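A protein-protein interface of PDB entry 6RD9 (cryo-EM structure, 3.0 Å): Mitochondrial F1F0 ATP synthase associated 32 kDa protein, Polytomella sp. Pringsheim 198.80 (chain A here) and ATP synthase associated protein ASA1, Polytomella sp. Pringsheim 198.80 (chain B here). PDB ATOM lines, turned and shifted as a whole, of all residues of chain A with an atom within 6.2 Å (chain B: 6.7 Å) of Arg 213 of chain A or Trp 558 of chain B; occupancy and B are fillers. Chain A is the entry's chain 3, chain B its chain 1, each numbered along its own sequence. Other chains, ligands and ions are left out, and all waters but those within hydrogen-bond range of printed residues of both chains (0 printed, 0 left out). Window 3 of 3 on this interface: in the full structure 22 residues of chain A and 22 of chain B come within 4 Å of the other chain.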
ATOM      1  N   GLU A 173     -25.920  17.459  34.124  1.00  0.00           N
ATOM      2  CA  GLU A 173     -25.995  18.590  33.226  1.00  0.00           C
ATOM      3  C   GLU A 173     -24.748  19.440  33.333  1.00  0.00           C
ATOM      4  O   GLU A 173     -24.001  19.345  34.296  1.00  0.00           O
ATOM      5  CB  GLU A 173     -27.227  19.409  33.533  1.00  0.00           C
ATOM      6  CG  GLU A 173     -28.449  18.592  33.450  1.00  0.00           C
ATOM      7  CD  GLU A 173     -29.676  19.423  33.501  1.00  0.00           C
ATOM      8  OE1 GLU A 173     -29.790  20.246  34.431  1.00  0.00           O
ATOM      9  OE2 GLU A 173     -30.516  19.274  32.591  1.00  0.00           O
ATOM     10  N   ASN A 206     -25.000  16.367  26.698  1.00  0.00           N
ATOM     11  CA  ASN A 206     -25.595  17.642  27.033  1.00  0.00           C
ATOM     12  C   ASN A 206     -25.704  18.501  25.799  1.00  0.00           C
ATOM     13  O   ASN A 206     -24.975  18.307  24.831  1.00  0.00           O
ATOM     14  CB  ASN A 206     -24.792  18.360  28.080  1.00  0.00           C
ATOM     15  CG  ASN A 206     -25.200  17.989  29.440  1.00  0.00           C
ATOM     16  OD1 ASN A 206     -24.499  17.301  30.151  1.00  0.00           O
ATOM     17  ND2 ASN A 206     -26.351  18.460  29.831  1.00  0.00           N
ATOM     18  N   HIS A 207     -26.625  19.461  25.858  1.00  0.00           N
ATOM     19  CA  HIS A 207     -26.894  20.335  24.731  1.00  0.00           C
ATOM     20  C   HIS A 207     -25.665  21.144  24.383  1.00  0.00           C
ATOM     21  O   HIS A 207     -24.894  21.525  25.254  1.00  0.00           O
ATOM     22  CB  HIS A 207     -28.041  21.269  25.050  1.00  0.00           C
ATOM     23  CG  HIS A 207     -28.663  21.877  23.841  1.00  0.00           C
ATOM     24  ND1 HIS A 207     -28.170  23.006  23.244  1.00  0.00           N
ATOM     25  CD2 HIS A 207     -29.716  21.494  23.096  1.00  0.00           C
ATOM     26  CE1 HIS A 207     -28.899  23.304  22.191  1.00  0.00           C
ATOM     27  NE2 HIS A 207     -29.841  22.395  22.076  1.00  0.00           N
ATOM     28  N   TYR A 208     -25.455  21.375  23.098  1.00  0.00           N
ATOM     29  CA  TYR A 208     -24.200  21.970  22.686  1.00  0.00           C
ATOM     30  C   TYR A 208     -24.133  23.455  22.963  1.00  0.00           C
ATOM     31  O   TYR A 208     -23.049  24.028  22.876  1.00  0.00           O
ATOM     32  CB  TYR A 208     -23.955  21.671  21.217  1.00  0.00           C
ATOM     33  CG  TYR A 208     -24.668  22.500  20.200  1.00  0.00           C
ATOM     34  CD1 TYR A 208     -26.026  22.425  20.039  1.00  0.00           C
ATOM     35  CD2 TYR A 208     -23.961  23.301  19.352  1.00  0.00           C
ATOM     36  CE1 TYR A 208     -26.653  23.178  19.095  1.00  0.00           C
ATOM     37  CE2 TYR A 208     -24.574  24.037  18.414  1.00  0.00           C
ATOM     38  CZ  TYR A 208     -25.914  23.976  18.291  1.00  0.00           C
ATOM     39  OH  TYR A 208     -26.492  24.732  17.328  1.00  0.00           O
ATOM     40  N   LEU A 209     -25.240  24.082  23.324  1.00  0.00           N
ATOM     41  CA  LEU A 209     -25.255  25.465  23.749  1.00  0.00           C
ATOM     42  C   LEU A 209     -25.330  25.597  25.243  1.00  0.00           C
ATOM     43  O   LEU A 209     -25.537  26.694  25.736  1.00  0.00           O
ATOM     44  CB  LEU A 209     -26.430  26.206  23.141  1.00  0.00           C
ATOM     45  CG  LEU A 209     -26.612  26.196  21.647  1.00  0.00           C
ATOM     46  CD1 LEU A 209     -27.926  26.805  21.365  1.00  0.00           C
ATOM     47  CD2 LEU A 209     -25.540  26.985  21.014  1.00  0.00           C
ATOM     48  N   ALA A 210     -25.216  24.527  25.962  1.00  0.00           N
ATOM     49  CA  ALA A 210     -25.100  24.617  27.403  1.00  0.00           C
ATOM     50  C   ALA A 210     -23.829  25.307  27.899  1.00  0.00           C
ATOM     51  O   ALA A 210     -23.862  25.848  29.004  1.00  0.00           O
ATOM     52  CB  ALA A 210     -25.214  23.232  28.026  1.00  0.00           C
ATOM     53  N   PRO A 211     -22.693  25.306  27.181  1.00  0.00           N
ATOM     54  CA  PRO A 211     -21.631  26.241  27.557  1.00  0.00           C
ATOM     55  C   PRO A 211     -21.973  27.703  27.396  1.00  0.00           C
ATOM     56  O   PRO A 211     -21.394  28.537  28.092  1.00  0.00           O
ATOM     57  CB  PRO A 211     -20.505  25.839  26.614  1.00  0.00           C
ATOM     58  CG  PRO A 211     -20.660  24.464  26.504  1.00  0.00           C
ATOM     59  CD  PRO A 211     -22.085  24.200  26.415  1.00  0.00           C
ATOM     60  N   VAL A 212     -22.880  28.049  26.492  1.00  0.00           N
ATOM     61  CA  VAL A 212     -23.234  29.442  26.271  1.00  0.00           C
ATOM     62  C   VAL A 212     -24.025  29.997  27.448  1.00  0.00           C
ATOM     63  O   VAL A 212     -23.969  31.193  27.743  1.00  0.00           O
ATOM     64  CB  VAL A 212     -23.989  29.521  24.939  1.00  0.00           C
ATOM     65  CG1 VAL A 212     -24.334  30.891  24.598  1.00  0.00           C
ATOM     66  CG2 VAL A 212     -23.131  28.976  23.860  1.00  0.00           C
ATOM     67  N   ARG A 213     -24.725  29.141  28.171  1.00  0.00           N
ATOM     68  CA  ARG A 213     -25.469  29.516  29.356  1.00  0.00           C
ATOM     69  C   ARG A 213     -24.661  29.420  30.628  1.00  0.00           C
ATOM     70  O   ARG A 213     -25.246  29.429  31.709  1.00  0.00           O
ATOM     71  CB  ARG A 213     -26.692  28.620  29.497  1.00  0.00           C
ATOM     72  CG  ARG A 213     -27.841  29.009  28.632  1.00  0.00           C
ATOM     73  CD  ARG A 213     -28.697  30.020  29.328  1.00  0.00           C
ATOM     74  NE  ARG A 213     -29.915  30.234  28.587  1.00  0.00           N
ATOM     75  CZ  ARG A 213     -30.026  31.098  27.598  1.00  0.00           C
ATOM     76  NH1 ARG A 213     -31.169  31.223  26.955  1.00  0.00           N
ATOM     77  NH2 ARG A 213     -28.996  31.849  27.260  1.00  0.00           N
ATOM     78  N   ALA A 214     -23.342  29.327  30.547  1.00  0.00           N
ATOM     79  CA  ALA A 214     -22.559  28.924  31.707  1.00  0.00           C
ATOM     80  C   ALA A 214     -21.915  30.083  32.440  1.00  0.00           C
ATOM     81  O   ALA A 214     -21.858  30.073  33.671  1.00  0.00           O
ATOM     82  CB  ALA A 214     -21.471  27.941  31.298  1.00  0.00           C
ATOM     83  N   GLY A 215     -21.409  31.070  31.730  1.00  0.00           N
ATOM     84  CA  GLY A 215     -20.660  32.101  32.408  1.00  0.00           C
ATOM     85  C   GLY A 215     -19.205  31.715  32.425  1.00  0.00           C
ATOM     86  O   GLY A 215     -18.846  30.657  32.937  1.00  0.00           O
ATOM     87  N   GLU A 218     -16.762  29.916  35.062  1.00  0.00           N
ATOM     88  CA  GLU A 218     -16.876  28.498  35.349  1.00  0.00           C
ATOM     89  C   GLU A 218     -16.278  27.652  34.256  1.00  0.00           C
ATOM     90  O   GLU A 218     -15.827  26.539  34.523  1.00  0.00           O
ATOM     91  CB  GLU A 218     -18.336  28.102  35.521  1.00  0.00           C
ATOM     92  CG  GLU A 218     -18.894  28.373  36.876  1.00  0.00           C
ATOM     93  CD  GLU A 218     -20.364  28.073  36.944  1.00  0.00           C
ATOM     94  OE1 GLU A 218     -21.076  28.399  35.977  1.00  0.00           O
ATOM     95  OE2 GLU A 218     -20.810  27.502  37.958  1.00  0.00           O
ATOM     96  N   GLY A 243     -18.593  28.757  24.832  1.00  0.00           N
ATOM     97  CA  GLY A 243     -19.074  29.636  25.855  1.00  0.00           C
ATOM     98  C   GLY A 243     -18.209  30.819  26.169  1.00  0.00           C
ATOM     99  O   GLY A 243     -18.430  31.465  27.192  1.00  0.00           O
ATOM    100  N   LYS A 251     -20.402  39.869  31.026  1.00  0.00           N
ATOM    101  CA  LYS A 251     -21.149  39.750  32.267  1.00  0.00           C
ATOM    102  C   LYS A 251     -20.248  39.600  33.476  1.00  0.00           C
ATOM    103  O   LYS A 251     -20.754  39.445  34.590  1.00  0.00           O
ATOM    104  CB  LYS A 251     -22.105  38.564  32.191  1.00  0.00           C
ATOM    105  CG  LYS A 251     -23.085  38.686  31.060  1.00  0.00           C
ATOM    106  CD  LYS A 251     -23.926  37.453  30.904  1.00  0.00           C
ATOM    107  CE  LYS A 251     -24.776  37.562  29.660  1.00  0.00           C
ATOM    108  NZ  LYS A 251     -25.717  36.435  29.536  1.00  0.00           N
ATOM    109  N   ILE B 553     -34.265  13.503  24.091  1.00  0.00           N
ATOM    110  CA  ILE B 553     -35.301  14.153  24.870  1.00  0.00           C
ATOM    111  C   ILE B 553     -34.698  15.054  25.926  1.00  0.00           C
ATOM    112  O   ILE B 553     -35.227  16.123  26.197  1.00  0.00           O
ATOM    113  CB  ILE B 553     -36.195  13.053  25.454  1.00  0.00           C
ATOM    114  CG1 ILE B 553     -36.913  12.330  24.332  1.00  0.00           C
ATOM    115  CG2 ILE B 553     -37.143  13.556  26.445  1.00  0.00           C
ATOM    116  CD1 ILE B 553     -37.669  13.203  23.429  1.00  0.00           C
ATOM    117  N   LYS B 554     -33.560  14.676  26.493  1.00  0.00           N
ATOM    118  CA  LYS B 554     -32.879  15.497  27.484  1.00  0.00           C
ATOM    119  C   LYS B 554     -32.358  16.787  26.885  1.00  0.00           C
ATOM    120  O   LYS B 554     -32.418  17.834  27.523  1.00  0.00           O
ATOM    121  CB  LYS B 554     -31.730  14.713  28.089  1.00  0.00           C
ATOM    122  CG  LYS B 554     -31.015  15.405  29.192  1.00  0.00           C
ATOM    123  CD  LYS B 554     -29.623  14.923  29.288  1.00  0.00           C
ATOM    124  CE  LYS B 554     -28.900  15.611  30.369  1.00  0.00           C
ATOM    125  NZ  LYS B 554     -27.475  15.267  30.297  1.00  0.00           N
ATOM    126  N   LYS B 555     -31.847  16.738  25.664  1.00  0.00           N
ATOM    127  CA  LYS B 555     -31.341  17.930  25.010  1.00  0.00           C
ATOM    128  C   LYS B 555     -32.441  18.769  24.399  1.00  0.00           C
ATOM    129  O   LYS B 555     -32.262  19.968  24.236  1.00  0.00           O
ATOM    130  CB  LYS B 555     -30.368  17.550  23.917  1.00  0.00           C
ATOM    131  CG  LYS B 555     -29.134  16.922  24.387  1.00  0.00           C
ATOM    132  CD  LYS B 555     -28.260  16.637  23.242  1.00  0.00           C
ATOM    133  CE  LYS B 555     -27.595  15.353  23.406  1.00  0.00           C
ATOM    134  NZ  LYS B 555     -26.431  15.299  22.546  1.00  0.00           N
ATOM    135  N   ILE B 556     -33.544  18.158  23.986  1.00  0.00           N
ATOM    136  CA  ILE B 556     -34.708  18.909  23.539  1.00  0.00           C
ATOM    137  C   ILE B 556     -35.316  19.673  24.696  1.00  0.00           C
ATOM    138  O   ILE B 556     -35.667  20.844  24.566  1.00  0.00           O
ATOM    139  CB  ILE B 556     -35.722  17.957  22.892  1.00  0.00           C
ATOM    140  CG1 ILE B 556     -35.312  17.602  21.480  1.00  0.00           C
ATOM    141  CG2 ILE B 556     -37.054  18.551  22.835  1.00  0.00           C
ATOM    142  CD1 ILE B 556     -36.045  16.457  20.968  1.00  0.00           C
ATOM    143  N   ASP B 557     -35.407  19.038  25.858  1.00  0.00           N
ATOM    144  CA  ASP B 557     -35.908  19.688  27.056  1.00  0.00           C
ATOM    145  C   ASP B 557     -35.005  20.785  27.553  1.00  0.00           C
ATOM    146  O   ASP B 557     -35.451  21.609  28.339  1.00  0.00           O
ATOM    147  CB  ASP B 557     -36.062  18.687  28.179  1.00  0.00           C
ATOM    148  CG  ASP B 557     -37.177  17.746  27.959  1.00  0.00           C
ATOM    149  OD1 ASP B 557     -37.817  17.834  26.908  1.00  0.00           O
ATOM    150  OD2 ASP B 557     -37.423  16.916  28.842  1.00  0.00           O
ATOM    151  N   TRP B 558     -33.738  20.787  27.180  1.00  0.00           N
ATOM    152  CA  TRP B 558     -32.880  21.890  27.568  1.00  0.00           C
ATOM    153  C   TRP B 558     -33.237  23.141  26.803  1.00  0.00           C
ATOM    154  O   TRP B 558     -33.120  24.241  27.329  1.00  0.00           O
ATOM    155  CB  TRP B 558     -31.416  21.538  27.351  1.00  0.00           C
ATOM    156  CG  TRP B 558     -30.489  22.573  27.850  1.00  0.00           C
ATOM    157  CD1 TRP B 558     -29.951  22.641  29.069  1.00  0.00           C
ATOM    158  CD2 TRP B 558     -30.002  23.704  27.131  1.00  0.00           C
ATOM    159  NE1 TRP B 558     -29.159  23.741  29.171  1.00  0.00           N
ATOM    160  CE2 TRP B 558     -29.176  24.402  27.979  1.00  0.00           C
ATOM    161  CE3 TRP B 558     -30.193  24.188  25.844  1.00  0.00           C
ATOM    162  CZ2 TRP B 558     -28.565  25.556  27.604  1.00  0.00           C
ATOM    163  CZ3 TRP B 558     -29.593  25.310  25.480  1.00  0.00           C
ATOM    164  CH2 TRP B 558     -28.786  25.991  26.342  1.00  0.00           C
ATOM    165  N   GLU B 559     -33.654  23.003  25.557  1.00  0.00           N
ATOM    166  CA  GLU B 559     -34.035  24.171  24.788  1.00  0.00           C
ATOM    167  C   GLU B 559     -35.344  24.750  25.278  1.00  0.00           C
ATOM    168  O   GLU B 559     -35.531  25.962  25.249  1.00  0.00           O
ATOM    169  CB  GLU B 559     -34.149  23.807  23.331  1.00  0.00           C
ATOM    170  CG  GLU B 559     -32.990  23.089  22.831  1.00  0.00           C
ATOM    171  CD  GLU B 559     -32.955  23.059  21.351  1.00  0.00           C
ATOM    172  OE1 GLU B 559     -33.647  23.872  20.738  1.00  0.00           O
ATOM    173  OE2 GLU B 559     -32.247  22.220  20.788  1.00  0.00           O
ATOM    174  N   THR B 560     -36.275  23.911  25.703  1.00  0.00           N
ATOM    175  CA  THR B 560     -37.518  24.429  26.245  1.00  0.00           C
ATOM    176  C   THR B 560     -37.292  25.072  27.597  1.00  0.00           C
ATOM    177  O   THR B 560     -37.888  26.100  27.896  1.00  0.00           O
ATOM    178  CB  THR B 560     -38.551  23.321  26.346  1.00  0.00           C
ATOM    179  OG1 THR B 560     -38.586  22.605  25.117  1.00  0.00           O
ATOM    180  CG2 THR B 560     -39.886  23.877  26.568  1.00  0.00           C
ATOM    181  N   THR B 561     -36.415  24.500  28.412  1.00  0.00           N
ATOM    182  CA  THR B 561     -36.150  25.057  29.729  1.00  0.00           C
ATOM    183  C   THR B 561     -35.429  26.379  29.627  1.00  0.00           C
ATOM    184  O   THR B 561     -35.750  27.329  30.339  1.00  0.00           O
ATOM    185  CB  THR B 561     -35.330  24.075  30.536  1.00  0.00           C
ATOM    186  OG1 THR B 561     -36.021  22.835  30.589  1.00  0.00           O
ATOM    187  CG2 THR B 561     -35.131  24.551  31.913  1.00  0.00           C
ATOM    188  N   ASN B 562     -34.481  26.471  28.713  1.00  0.00           N
ATOM    189  CA  ASN B 562     -33.661  27.654  28.552  1.00  0.00           C
ATOM    190  C   ASN B 562     -34.137  28.535  27.433  1.00  0.00           C
ATOM    191  O   ASN B 562     -33.318  29.130  26.741  1.00  0.00           O
ATOM    192  CB  ASN B 562     -32.224  27.247  28.331  1.00  0.00           C
ATOM    193  CG  ASN B 562     -31.675  26.579  29.514  1.00  0.00           C
ATOM    194  OD1 ASN B 562     -31.850  25.398  29.688  1.00  0.00           O
ATOM    195  ND2 ASN B 562     -31.052  27.332  30.379  1.00  0.00           N
ATOM    196  N   ALA B 563     -35.443  28.568  27.216  1.00  0.00           N
ATOM    197  CA  ALA B 563     -36.151  29.573  26.441  1.00  0.00           C
ATOM    198  C   ALA B 563     -35.722  29.627  24.995  1.00  0.00           C
ATOM    199  O   ALA B 563     -35.849  30.659  24.350  1.00  0.00           O
ATOM    200  CB  ALA B 563     -36.003  30.948  27.075  1.00  0.00           C
ATOM    201  N   LEU B 564     -35.195  28.540  24.473  1.00  0.00           N
ATOM    202  CA  LEU B 564     -34.789  28.447  23.085  1.00  0.00           C
ATOM    203  C   LEU B 564     -35.634  27.426  22.359  1.00  0.00           C
ATOM    204  O   LEU B 564     -35.142  26.699  21.510  1.00  0.00           O
ATOM    205  CB  LEU B 564     -33.329  28.057  22.961  1.00  0.00           C
ATOM    206  CG  LEU B 564     -32.217  28.873  23.577  1.00  0.00           C
ATOM    207  CD1 LEU B 564     -31.033  28.000  23.624  1.00  0.00           C
ATOM    208  CD2 LEU B 564     -31.933  30.035  22.713  1.00  0.00           C
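Arg 213 of chain A touches two residues of chain B.
Trp 558 of chain B touches just these residues of chain A: His 207 (3.4 Å), Leu 209 (3.4 Å), Ala 210 (3.6 Å) and Arg 213 (3.7 Å).
Of the printed residues of chain B, Asn 206 of chain A touches Lys 554.
Of the printed residues of chain B, His 207 of chain A touches Lys 555, Trp 558 and Glu 559.
Pro 211 of chain A touches none of the printed residues of chain B.
The nearest residue of chain A that does not touch Trp 558 of chain B is Glu 173 of chain A (4.9 Å).
Of the 14 printed residues of chain A, 5 touch a printed residue of chain B.
Hydrophobic or aromatic side chains of chain A that line the printed part of chain B: His 207 and Leu 209.
Of the 12 printed residues of chain B, 5 touch a printed residue of chain A.
Printed residues of chain B that touch a printed residue of chain A: Lys 554, Lys 555, Trp 558, Glu 559 and Asn 562.
Hydrophobic or aromatic side chains of chain B that line the printed part of chain A: Trp 558.
Among the printed residues, 8 pairs touch across the chains.
Among the printed residues, no Asp or Glu carboxylate lies within 4 Å of a Lys or Arg side-chain nitrogen of the other chain.
Among the printed residues, pairs that only touch across the chains: His 207 of chain A with Lys 555 of chain B (3.2 Å), Leu 209 of chain A with Trp 558 of chain B (3.4 Å), His 207 of chain A with Trp 558 of chain B (3.4 Å), Ala 210 of chain A with Trp 558 of chain B (3.6 Å) and Arg 213 of chain A with Trp 558 of chain B (3.7 Å).
O of Trp 558 of chain B lies close to OD1 of Asn 562 of chain B, at 2.9 Å.
O of Glu 559 of chain B lies within hydrogen-bond range of N of Leu 564 of chain B.
A ring nitrogen (ND1) of His 207 of chain A sits at hydrogen-bond distance from the backbone NH (N) of Leu 209 of chain A (3.1 Å).
The backbone carbonyl oxygen (O) of Asn 562 of chain B is in hydrogen-bond range of the guanidinium group (NH1) of Arg 213 of chain A, at 3.0 Å.
NZ of Lys 554 of chain B sits close to ND2 of Asn 206 of chain A.
A ring nitrogen (NE2) of His 207 of chain A is in hydrogen-bond range of the side-chain carboxylate of Glu 559 of chain B.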
